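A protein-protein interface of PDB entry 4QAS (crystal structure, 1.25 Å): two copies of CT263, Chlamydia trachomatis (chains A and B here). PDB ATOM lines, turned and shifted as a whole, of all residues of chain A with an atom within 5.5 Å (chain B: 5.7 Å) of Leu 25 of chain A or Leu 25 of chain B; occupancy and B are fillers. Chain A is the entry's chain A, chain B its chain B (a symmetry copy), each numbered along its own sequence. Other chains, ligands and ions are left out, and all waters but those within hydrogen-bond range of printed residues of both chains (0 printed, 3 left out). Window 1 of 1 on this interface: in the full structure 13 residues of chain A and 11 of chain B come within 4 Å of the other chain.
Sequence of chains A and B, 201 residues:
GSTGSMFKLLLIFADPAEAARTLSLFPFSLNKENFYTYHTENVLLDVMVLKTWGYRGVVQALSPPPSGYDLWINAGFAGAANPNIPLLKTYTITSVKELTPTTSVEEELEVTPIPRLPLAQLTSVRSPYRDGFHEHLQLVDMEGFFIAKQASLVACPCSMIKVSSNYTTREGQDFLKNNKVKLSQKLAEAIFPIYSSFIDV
Among the printed residues, pairs that only touch across the chains: Arg 21 of chain A with Leu 25 of chain B (3.5 Å), Arg 21 of chain A with Pro 27 of chain B (3.6 Å), Leu 25 of chain A with Leu 25 of chain B (3.9 Å), Leu 25 of chain A with Phe 192 of chain B (3.6 Å), Phe 26 of chain A with Gln 185 of chain B (3.5 Å), Phe 26 of chain A with Glu 189 of chain B (3.5 Å), Pro 27 of chain A with Arg 21 of chain B (3.6 Å), Pro 27 of chain A with Gln 185 of chain B (3.7 Å), Gln 185 of chain A with Phe 26 of chain B (3.4 Å), Gln 185 of chain A with Pro 27 of chain B (3.5 Å), Gln 185 of chain A with Phe 192 of chain B (3.8 Å), Ala 188 of chain A with Phe 192 of chain B (3.7 Å), Glu 189 of chain A with Phe 26 of chain B (3.8 Å), Glu 189 of chain A with Phe 192 of chain B (3.5 Å), Phe 192 of chain A with Glu 189 of chain B (3.6 Å) and Phe 192 of chain A with Phe 192 of chain B (3.5 Å).
Printed residues of chain B within 4 Å of Arg 21 of chain A: Ser 24 (3.0 Å), Leu 25 (3.5 Å), Phe 26 (3.2 Å) and Pro 27 (3.6 Å). Leu 25 of chain A touches four residues of chain B. Of the printed residues of chain A, Arg 21 of chain B touches Ser 24, Leu 25, Phe 26 and Pro 27. Thr 22 of chain B touches none of the printed residues of chain A. Leu 25 of chain B touches three residues of chain A. Printed residues of chain A within 4 Å of Gln 185 of chain B: Leu 25, Phe 26 and Pro 27.
Arg 21 of chain A touches Ser 24 of chain B, and with the chains exchanged Ser 24 of chain A touches Arg 21 of chain B. Arg 21 of chain A touches Pro 27 of chain B, and with the chains exchanged Pro 27 of chain A touches Arg 21 of chain B. Ala 188 of chain A touches Phe 192 of chain B, but with the chains exchanged Phe 192 of chain A does not touch Ala 188 of chain B (5.7 Å). Phe 192 of chain A touches its own counterpart, Phe 192 of chain B. Positions printed for both chains: 21, 22, 23, 24, 25, 26, 27, 28, 185, 188, 189, 191 and 192.
The guanidinium group (NH2) of Arg 21 of chain B is in hydrogen-bond range of the backbone carbonyl oxygen (O) of Ser 24 of chain A (2.9 Å). OG of Ser 24 of chain A is in hydrogen-bond range of O of Ser 24 of chain B. The backbone carbonyl oxygen of Leu 25 of chain A is in hydrogen-bond range of the side-chain amide nitrogen of Gln 185 of chain B, at 3.1 Å. The guanidinium group (NH2) of Arg 21 of chain B sits close to the backbone NH (N) of Phe 26 of chain A, 3.3 Å away. The guanidinium group (NH2) of Arg 21 of chain A sits close to the backbone carbonyl oxygen (O) of Phe 26 of chain B, 3.5 Å away. The side-chain amide nitrogen (NE2) of Gln 185 of chain A is in hydrogen-bond range of the backbone carbonyl oxygen (O) of Leu 25 of chain B. The backbone carbonyl oxygen (O) of Leu 25 of chain A sits at hydrogen-bond distance from the guanidinium group (NH2) of Arg 21 of chain B, at 3.1 Å. The guanidinium group (NH2) of Arg 21 of chain A is in hydrogen-bond range of the backbone carbonyl oxygen (O) of Ser 24 of chain B.
Of the 13 printed residues of chain B, 8 touch a printed residue of chain A. Hydrophobic or aromatic side chains of chain B that line the printed part of chain A: Leu 25, Phe 26, Pro 27 and Phe 192. Hydrophobic or aromatic side chains of chain A that line the printed part of chain B: Leu 25, Phe 26, Pro 27 and Phe 192. Along chain A the printed residues that touch a printed residue of chain B span positions 21 to 192. Among the printed residues, no Asp or Glu carboxylate lies within 4 Å of a Lys or Arg side-chain nitrogen of the other chain.
The side-chain amide oxygen (OE1) of Gln 185 of chain A is in hydrogen-bond range of the guanidinium group (NE) of Arg 21 of chain A, 2.9 Å away. NE of Arg 21 of chain B is in hydrogen-bond range of OE1 of Gln 185 of chain B, at 2.7 Å. The side-chain amide nitrogen (NE2) of Gln 185 of chain B lies within hydrogen-bond range of the side-chain carboxylate (OE1) of Glu 189 of chain B (3.0 Å). The side-chain amide nitrogen (NE2) of Gln 185 of chain A lies within hydrogen-bond range of the side-chain carboxylate (OE2) of Glu 189 of chain A, at 3.1 Å.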
ATOM      1  N   ARG A  21     -15.691   8.690  -9.755  1.00  0.00           N
ATOM      2  CA  ARG A  21     -14.306   8.258  -9.549  1.00  0.00           C
ATOM      3  C   ARG A  21     -14.040   6.899 -10.181  1.00  0.00           C
ATOM      4  O   ARG A  21     -12.933   6.657 -10.663  1.00  0.00           O
ATOM      5  CB  ARG A  21     -13.922   8.298  -8.071  1.00  0.00           C
ATOM      6  CG  ARG A  21     -14.002   9.697  -7.439  1.00  0.00           C
ATOM      7  CD  ARG A  21     -13.144  10.753  -8.126  1.00  0.00           C
ATOM      8  NE  ARG A  21     -11.815  10.273  -8.407  1.00  0.00           N
ATOM      9  CZ  ARG A  21     -11.000  10.807  -9.293  1.00  0.00           C
ATOM     10  NH1 ARG A  21     -11.302  11.967  -9.841  1.00  0.00           N
ATOM     11  NH2 ARG A  21      -9.826  10.256  -9.560  1.00  0.00           N
ATOM     12  N   THR A  22     -15.041   6.031 -10.267  1.00  0.00           N
ATOM     13  CA  THR A  22     -14.851   4.785 -11.000  1.00  0.00           C
ATOM     14  C   THR A  22     -14.640   5.041 -12.485  1.00  0.00           C
ATOM     15  O   THR A  22     -13.803   4.387 -13.120  1.00  0.00           O
ATOM     16  CB  THR A  22     -16.039   3.857 -10.773  1.00  0.00           C
ATOM     17  OG1 THR A  22     -16.074   3.478  -9.386  1.00  0.00           O
ATOM     18  CG2 THR A  22     -15.917   2.601 -11.615  1.00  0.00           C
ATOM     19  N   LEU A  23     -15.349   6.012 -13.053  1.00  0.00           N
ATOM     20  CA  LEU A  23     -15.167   6.340 -14.452  1.00  0.00           C
ATOM     21  C   LEU A  23     -13.790   6.925 -14.716  1.00  0.00           C
ATOM     22  O   LEU A  23     -13.309   6.823 -15.846  1.00  0.00           O
ATOM     23  CB  LEU A  23     -16.262   7.289 -14.915  1.00  0.00           C
ATOM     24  CG  LEU A  23     -17.677   6.686 -15.039  1.00  0.00           C
ATOM     25  CD1 LEU A  23     -18.699   7.785 -15.240  1.00  0.00           C
ATOM     26  CD2 LEU A  23     -17.719   5.697 -16.175  1.00  0.00           C
ATOM     27  N   SER A  24     -13.124   7.489 -13.698  1.00  0.00           N
ATOM     28  CA  SER A  24     -11.756   7.963 -13.862  1.00  0.00           C
ATOM     29  C   SER A  24     -10.726   6.831 -13.800  1.00  0.00           C
ATOM     30  O   SER A  24      -9.613   7.007 -14.271  1.00  0.00           O
ATOM     31  CB  SER A  24     -11.468   9.016 -12.789  1.00  0.00           C
ATOM     32  OG  SER A  24     -10.272   9.668 -13.064  1.00  0.00           O
ATOM     33  N   LEU A  25     -11.066   5.694 -13.210  1.00  0.00           N
ATOM     34  CA  LEU A  25     -10.083   4.627 -12.988  1.00  0.00           C
ATOM     35  C   LEU A  25      -9.618   3.962 -14.263  1.00  0.00           C
ATOM     36  O   LEU A  25      -8.513   3.428 -14.297  1.00  0.00           O
ATOM     37  CB  LEU A  25     -10.702   3.508 -12.182  1.00  0.00           C
ATOM     38  CG  LEU A  25     -11.004   3.700 -10.741  1.00  0.00           C
ATOM     39  CD1 LEU A  25     -11.496   2.313 -10.226  1.00  0.00           C
ATOM     40  CD2 LEU A  25      -9.784   4.165  -9.998  1.00  0.00           C
ATOM     41  N   PHE A  26     -10.469   3.906 -15.295  1.00  0.00           N
ATOM     42  CA  PHE A  26     -10.176   3.239 -16.550  1.00  0.00           C
ATOM     43  C   PHE A  26     -10.458   4.200 -17.690  1.00  0.00           C
ATOM     44  O   PHE A  26     -11.315   5.089 -17.546  1.00  0.00           O
ATOM     45  CB  PHE A  26     -11.047   1.978 -16.728  1.00  0.00           C
ATOM     46  CG  PHE A  26     -10.923   1.004 -15.619  1.00  0.00           C
ATOM     47  CD1 PHE A  26      -9.852   0.124 -15.571  1.00  0.00           C
ATOM     48  CD2 PHE A  26     -11.858   0.959 -14.636  1.00  0.00           C
ATOM     49  CE1 PHE A  26      -9.736  -0.775 -14.535  1.00  0.00           C
ATOM     50  CE2 PHE A  26     -11.753   0.068 -13.609  1.00  0.00           C
ATOM     51  CZ  PHE A  26     -10.678  -0.812 -13.568  1.00  0.00           C
ATOM     52  N   PRO A  27      -9.812   4.030 -18.803  1.00  0.00           N
ATOM     53  CA  PRO A  27     -10.049   4.921 -19.964  1.00  0.00           C
ATOM     54  C   PRO A  27     -11.299   4.494 -20.731  1.00  0.00           C
ATOM     55  O   PRO A  27     -11.250   4.007 -21.857  1.00  0.00           O
ATOM     56  CB  PRO A  27      -8.750   4.781 -20.772  1.00  0.00           C
ATOM     57  CG  PRO A  27      -8.270   3.419 -20.455  1.00  0.00           C
ATOM     58  CD  PRO A  27      -8.627   3.173 -19.031  1.00  0.00           C
ATOM     59  N   PHE A  28     -12.451   4.674 -20.088  1.00  0.00           N
ATOM     60  CA  PHE A  28     -13.732   4.352 -20.704  1.00  0.00           C
ATOM     61  C   PHE A  28     -13.984   5.230 -21.919  1.00  0.00           C
ATOM     62  O   PHE A  28     -13.493   6.358 -22.022  1.00  0.00           O
ATOM     63  CB  PHE A  28     -14.859   4.629 -19.716  1.00  0.00           C
ATOM     64  CG  PHE A  28     -14.966   3.636 -18.588  1.00  0.00           C
ATOM     65  CD1 PHE A  28     -15.575   2.415 -18.775  1.00  0.00           C
ATOM     66  CD2 PHE A  28     -14.488   3.935 -17.333  1.00  0.00           C
ATOM     67  CE1 PHE A  28     -15.683   1.511 -17.754  1.00  0.00           C
ATOM     68  CE2 PHE A  28     -14.608   3.031 -16.296  1.00  0.00           C
ATOM     69  CZ  PHE A  28     -15.211   1.828 -16.507  1.00  0.00           C
ATOM     70  N   GLN A 185     -14.876   8.080  -4.462  1.00  0.00           N
ATOM     71  CA  GLN A 185     -13.550   7.485  -4.446  1.00  0.00           C
ATOM     72  C   GLN A 185     -13.543   6.175  -3.671  1.00  0.00           C
ATOM     73  O   GLN A 185     -12.872   5.216  -4.082  1.00  0.00           O
ATOM     74  CB  GLN A 185     -12.532   8.492  -3.896  1.00  0.00           C
ATOM     75  CG  GLN A 185     -11.132   7.983  -3.893  1.00  0.00           C
ATOM     76  CD  GLN A 185     -10.567   7.821  -5.278  1.00  0.00           C
ATOM     77  OE1 GLN A 185     -11.014   8.471  -6.239  1.00  0.00           O
ATOM     78  NE2 GLN A 185      -9.548   6.969  -5.417  1.00  0.00           N
ATOM     79  N   ALA A 188     -14.740   3.476  -5.953  1.00  0.00           N
ATOM     80  CA  ALA A 188     -13.739   3.103  -6.940  1.00  0.00           C
ATOM     81  C   ALA A 188     -12.701   2.192  -6.326  1.00  0.00           C
ATOM     82  O   ALA A 188     -12.276   1.206  -6.942  1.00  0.00           O
ATOM     83  CB  ALA A 188     -13.093   4.358  -7.530  1.00  0.00           C
ATOM     84  N   GLU A 189     -12.288   2.512  -5.094  1.00  0.00           N
ATOM     85  CA  GLU A 189     -11.287   1.710  -4.418  1.00  0.00           C
ATOM     86  C   GLU A 189     -11.792   0.307  -4.128  1.00  0.00           C
ATOM     87  O   GLU A 189     -11.009  -0.651  -4.117  1.00  0.00           O
ATOM     88  CB  GLU A 189     -10.827   2.450  -3.164  1.00  0.00           C
ATOM     89  CG  GLU A 189     -10.047   3.699  -3.547  1.00  0.00           C
ATOM     90  CD  GLU A 189      -9.737   4.619  -2.396  1.00  0.00           C
ATOM     91  OE1 GLU A 189     -10.167   4.331  -1.253  1.00  0.00           O
ATOM     92  OE2 GLU A 189      -9.072   5.646  -2.644  1.00  0.00           O
ATOM     93  N   ILE A 191     -14.187  -1.250  -6.044  1.00  0.00           N
ATOM     94  CA  ILE A 191     -14.433  -1.926  -7.320  1.00  0.00           C
ATOM     95  C   ILE A 191     -13.152  -2.527  -7.877  1.00  0.00           C
ATOM     96  O   ILE A 191     -13.164  -3.623  -8.463  1.00  0.00           O
ATOM     97  CB  ILE A 191     -15.106  -0.947  -8.299  1.00  0.00           C
ATOM     98  CG1 ILE A 191     -16.561  -0.742  -7.858  1.00  0.00           C
ATOM     99  CG2 ILE A 191     -15.006  -1.477  -9.745  1.00  0.00           C
ATOM    100  CD1 ILE A 191     -17.277   0.366  -8.540  1.00  0.00           C
ATOM    101  N   PHE A 192     -12.031  -1.833  -7.728  1.00  0.00           N
ATOM    102  CA  PHE A 192     -10.834  -2.284  -8.422  1.00  0.00           C
ATOM    103  C   PHE A 192     -10.440  -3.720  -8.106  1.00  0.00           C
ATOM    104  O   PHE A 192     -10.157  -4.470  -9.051  1.00  0.00           O
ATOM    105  CB  PHE A 192      -9.666  -1.328  -8.198  1.00  0.00           C
ATOM    106  CG  PHE A 192      -8.460  -1.773  -8.918  1.00  0.00           C
ATOM    107  CD1 PHE A 192      -8.345  -1.563 -10.281  1.00  0.00           C
ATOM    108  CD2 PHE A 192      -7.497  -2.510  -8.273  1.00  0.00           C
ATOM    109  CE1 PHE A 192      -7.238  -2.035 -10.971  1.00  0.00           C
ATOM    110  CE2 PHE A 192      -6.404  -2.972  -8.948  1.00  0.00           C
ATOM    111  CZ  PHE A 192      -6.270  -2.738 -10.295  1.00  0.00           C
ATOM    112  N   ARG B  21      -2.275   7.984 -16.362  1.00  0.00           N
ATOM    113  CA  ARG B  21      -3.343   7.130 -15.859  1.00  0.00           C
ATOM    114  C   ARG B  21      -3.278   7.012 -14.340  1.00  0.00           C
ATOM    115  O   ARG B  21      -4.318   6.967 -13.687  1.00  0.00           O
ATOM    116  CB  ARG B  21      -3.352   5.767 -16.561  1.00  0.00           C
ATOM    117  CG  ARG B  21      -3.656   5.810 -18.054  1.00  0.00           C
ATOM    118  CD  ARG B  21      -4.992   6.401 -18.384  1.00  0.00           C
ATOM    119  NE  ARG B  21      -6.016   5.776 -17.545  1.00  0.00           N
ATOM    120  CZ  ARG B  21      -7.118   6.357 -17.128  1.00  0.00           C
ATOM    121  NH1 ARG B  21      -7.507   7.518 -17.640  1.00  0.00           N
ATOM    122  NH2 ARG B  21      -7.910   5.698 -16.293  1.00  0.00           N
ATOM    123  N   THR B  22      -2.081   6.974 -13.753  1.00  0.00           N
ATOM    124  CA  THR B  22      -1.977   7.001 -12.292  1.00  0.00           C
ATOM    125  C   THR B  22      -2.596   8.265 -11.717  1.00  0.00           C
ATOM    126  O   THR B  22      -3.293   8.217 -10.687  1.00  0.00           O
ATOM    127  CB  THR B  22      -0.512   6.842 -11.849  1.00  0.00           C
ATOM    128  OG1 THR B  22      -0.060   5.526 -12.169  1.00  0.00           O
ATOM    129  CG2 THR B  22      -0.379   7.047 -10.335  1.00  0.00           C
ATOM    130  N   LEU B  23      -2.390   9.401 -12.355  1.00  0.00           N
ATOM    131  CA  LEU B  23      -2.951  10.639 -11.853  1.00  0.00           C
ATOM    132  C   LEU B  23      -4.469  10.646 -11.953  1.00  0.00           C
ATOM    133  O   LEU B  23      -5.136  11.412 -11.249  1.00  0.00           O
ATOM    134  CB  LEU B  23      -2.318  11.807 -12.605  1.00  0.00           C
ATOM    135  CG  LEU B  23      -0.837  12.037 -12.254  1.00  0.00           C
ATOM    136  CD1 LEU B  23      -0.207  13.034 -13.216  1.00  0.00           C
ATOM    137  CD2 LEU B  23      -0.711  12.533 -10.845  1.00  0.00           C
ATOM    138  N   SER B  24      -5.053   9.791 -12.793  1.00  0.00           N
ATOM    139  CA  SER B  24      -6.509   9.684 -12.857  1.00  0.00           C
ATOM    140  C   SER B  24      -7.091   8.817 -11.750  1.00  0.00           C
ATOM    141  O   SER B  24      -8.304   8.764 -11.613  1.00  0.00           O
ATOM    142  CB  SER B  24      -6.985   9.156 -14.219  1.00  0.00           C
ATOM    143  OG  SER B  24      -6.346   9.851 -15.269  1.00  0.00           O
ATOM    144  N   LEU B  25      -6.259   8.144 -10.969  1.00  0.00           N
ATOM    145  CA  LEU B  25      -6.784   7.229  -9.951  1.00  0.00           C
ATOM    146  C   LEU B  25      -7.349   7.931  -8.728  1.00  0.00           C
ATOM    147  O   LEU B  25      -8.160   7.341  -8.015  1.00  0.00           O
ATOM    148  CB  LEU B  25      -5.665   6.348  -9.413  1.00  0.00           C
ATOM    149  CG  LEU B  25      -5.024   5.384 -10.391  1.00  0.00           C
ATOM    150  CD1 LEU B  25      -3.769   4.798  -9.723  1.00  0.00           C
ATOM    151  CD2 LEU B  25      -5.997   4.329 -10.814  1.00  0.00           C
ATOM    152  N   PHE B  26      -6.868   9.128  -8.426  1.00  0.00           N
ATOM    153  CA  PHE B  26      -7.233   9.817  -7.200  1.00  0.00           C
ATOM    154  C   PHE B  26      -7.523  11.257  -7.545  1.00  0.00           C
ATOM    155  O   PHE B  26      -6.931  11.801  -8.490  1.00  0.00           O
ATOM    156  CB  PHE B  26      -6.117   9.786  -6.151  1.00  0.00           C
ATOM    157  CG  PHE B  26      -5.662   8.402  -5.792  1.00  0.00           C
ATOM    158  CD1 PHE B  26      -6.304   7.680  -4.826  1.00  0.00           C
ATOM    159  CD2 PHE B  26      -4.556   7.837  -6.417  1.00  0.00           C
ATOM    160  CE1 PHE B  26      -5.879   6.418  -4.511  1.00  0.00           C
ATOM    161  CE2 PHE B  26      -4.138   6.581  -6.092  1.00  0.00           C
ATOM    162  CZ  PHE B  26      -4.798   5.880  -5.154  1.00  0.00           C
ATOM    163  N   PRO B  27      -8.352  11.946  -6.732  1.00  0.00           N
ATOM    164  CA  PRO B  27      -8.630  13.378  -6.940  1.00  0.00           C
ATOM    165  C   PRO B  27      -7.495  14.214  -6.354  1.00  0.00           C
ATOM    166  O   PRO B  27      -7.629  14.904  -5.305  1.00  0.00           O
ATOM    167  CB  PRO B  27      -9.962  13.561  -6.203  1.00  0.00           C
ATOM    168  CG  PRO B  27      -9.906  12.599  -5.104  1.00  0.00           C
ATOM    169  CD  PRO B  27      -9.220  11.385  -5.676  1.00  0.00           C
ATOM    170  N   PHE B  28      -6.330  14.132  -7.004  1.00  0.00           N
ATOM    171  CA  PHE B  28      -5.146  14.873  -6.581  1.00  0.00           C
ATOM    172  C   PHE B  28      -5.377  16.380  -6.633  1.00  0.00           C
ATOM    173  O   PHE B  28      -6.168  16.893  -7.415  1.00  0.00           O
ATOM    174  CB  PHE B  28      -3.969  14.580  -7.520  1.00  0.00           C
ATOM    175  CG  PHE B  28      -3.368  13.225  -7.357  1.00  0.00           C
ATOM    176  CD1 PHE B  28      -2.492  12.961  -6.350  1.00  0.00           C
ATOM    177  CD2 PHE B  28      -3.667  12.220  -8.244  1.00  0.00           C
ATOM    178  CE1 PHE B  28      -1.939  11.718  -6.193  1.00  0.00           C
ATOM    179  CE2 PHE B  28      -3.135  10.975  -8.109  1.00  0.00           C
ATOM    180  CZ  PHE B  28      -2.262  10.705  -7.086  1.00  0.00           C
ATOM    181  N   GLN B 185      -1.737   2.727 -18.107  1.00  0.00           N
ATOM    182  CA  GLN B 185      -2.765   2.092 -17.300  1.00  0.00           C
ATOM    183  C   GLN B 185      -2.199   0.904 -16.527  1.00  0.00           C
ATOM    184  O   GLN B 185      -2.597   0.656 -15.384  1.00  0.00           O
ATOM    185  CB  GLN B 185      -3.928   1.686 -18.196  1.00  0.00           C
ATOM    186  CG  GLN B 185      -5.084   1.024 -17.453  1.00  0.00           C
ATOM    187  CD  GLN B 185      -5.824   1.980 -16.532  1.00  0.00           C
ATOM    188  OE1 GLN B 185      -5.721   3.209 -16.665  1.00  0.00           O
ATOM    189  NE2 GLN B 185      -6.615   1.440 -15.623  1.00  0.00           N
ATOM    190  N   ALA B 188      -0.727   2.344 -13.468  1.00  0.00           N
ATOM    191  CA  ALA B 188      -1.768   2.773 -12.549  1.00  0.00           C
ATOM    192  C   ALA B 188      -2.383   1.587 -11.823  1.00  0.00           C
ATOM    193  O   ALA B 188      -2.658   1.667 -10.618  1.00  0.00           O
ATOM    194  CB  ALA B 188      -2.839   3.515 -13.331  1.00  0.00           C
ATOM    195  N   GLU B 189      -2.598   0.474 -12.530  1.00  0.00           N
ATOM    196  CA  GLU B 189      -3.210  -0.694 -11.903  1.00  0.00           C
ATOM    197  C   GLU B 189      -2.281  -1.377 -10.911  1.00  0.00           C
ATOM    198  O   GLU B 189      -2.756  -2.010  -9.969  1.00  0.00           O
ATOM    199  CB  GLU B 189      -3.656  -1.650 -12.998  1.00  0.00           C
ATOM    200  CG  GLU B 189      -4.816  -1.057 -13.744  1.00  0.00           C
ATOM    201  CD  GLU B 189      -5.296  -1.861 -14.906  1.00  0.00           C
ATOM    202  OE1 GLU B 189      -6.392  -1.514 -15.389  1.00  0.00           O
ATOM    203  OE2 GLU B 189      -4.561  -2.780 -15.360  1.00  0.00           O
ATOM    204  N   ILE B 191      -0.179   0.546  -9.073  1.00  0.00           N
ATOM    205  CA  ILE B 191      -0.064   1.529  -7.998  1.00  0.00           C
ATOM    206  C   ILE B 191      -1.322   1.570  -7.123  1.00  0.00           C
ATOM    207  O   ILE B 191      -1.236   1.756  -5.901  1.00  0.00           O
ATOM    208  CB  ILE B 191       0.261   2.901  -8.605  1.00  0.00           C
ATOM    209  CG1 ILE B 191       1.724   2.894  -9.080  1.00  0.00           C
ATOM    210  CG2 ILE B 191       0.022   4.021  -7.603  1.00  0.00           C
ATOM    211  CD1 ILE B 191       2.047   3.905 -10.110  1.00  0.00           C
ATOM    212  N   PHE B 192      -2.516   1.457  -7.722  1.00  0.00           N
ATOM    213  CA  PHE B 192      -3.758   1.618  -6.958  1.00  0.00           C
ATOM    214  C   PHE B 192      -3.807   0.711  -5.739  1.00  0.00           C
ATOM    215  O   PHE B 192      -4.150   1.199  -4.653  1.00  0.00           O
ATOM    216  CB  PHE B 192      -4.957   1.402  -7.903  1.00  0.00           C
ATOM    217  CG  PHE B 192      -6.260   2.082  -7.472  1.00  0.00           C
ATOM    218  CD1 PHE B 192      -6.318   3.424  -7.065  1.00  0.00           C
ATOM    219  CD2 PHE B 192      -7.452   1.351  -7.480  1.00  0.00           C
ATOM    220  CE1 PHE B 192      -7.509   4.004  -6.719  1.00  0.00           C
ATOM    221  CE2 PHE B 192      -8.646   1.937  -7.131  1.00  0.00           C
ATOM    222  CZ  PHE B 192      -8.679   3.264  -6.726  1.00  0.00           C
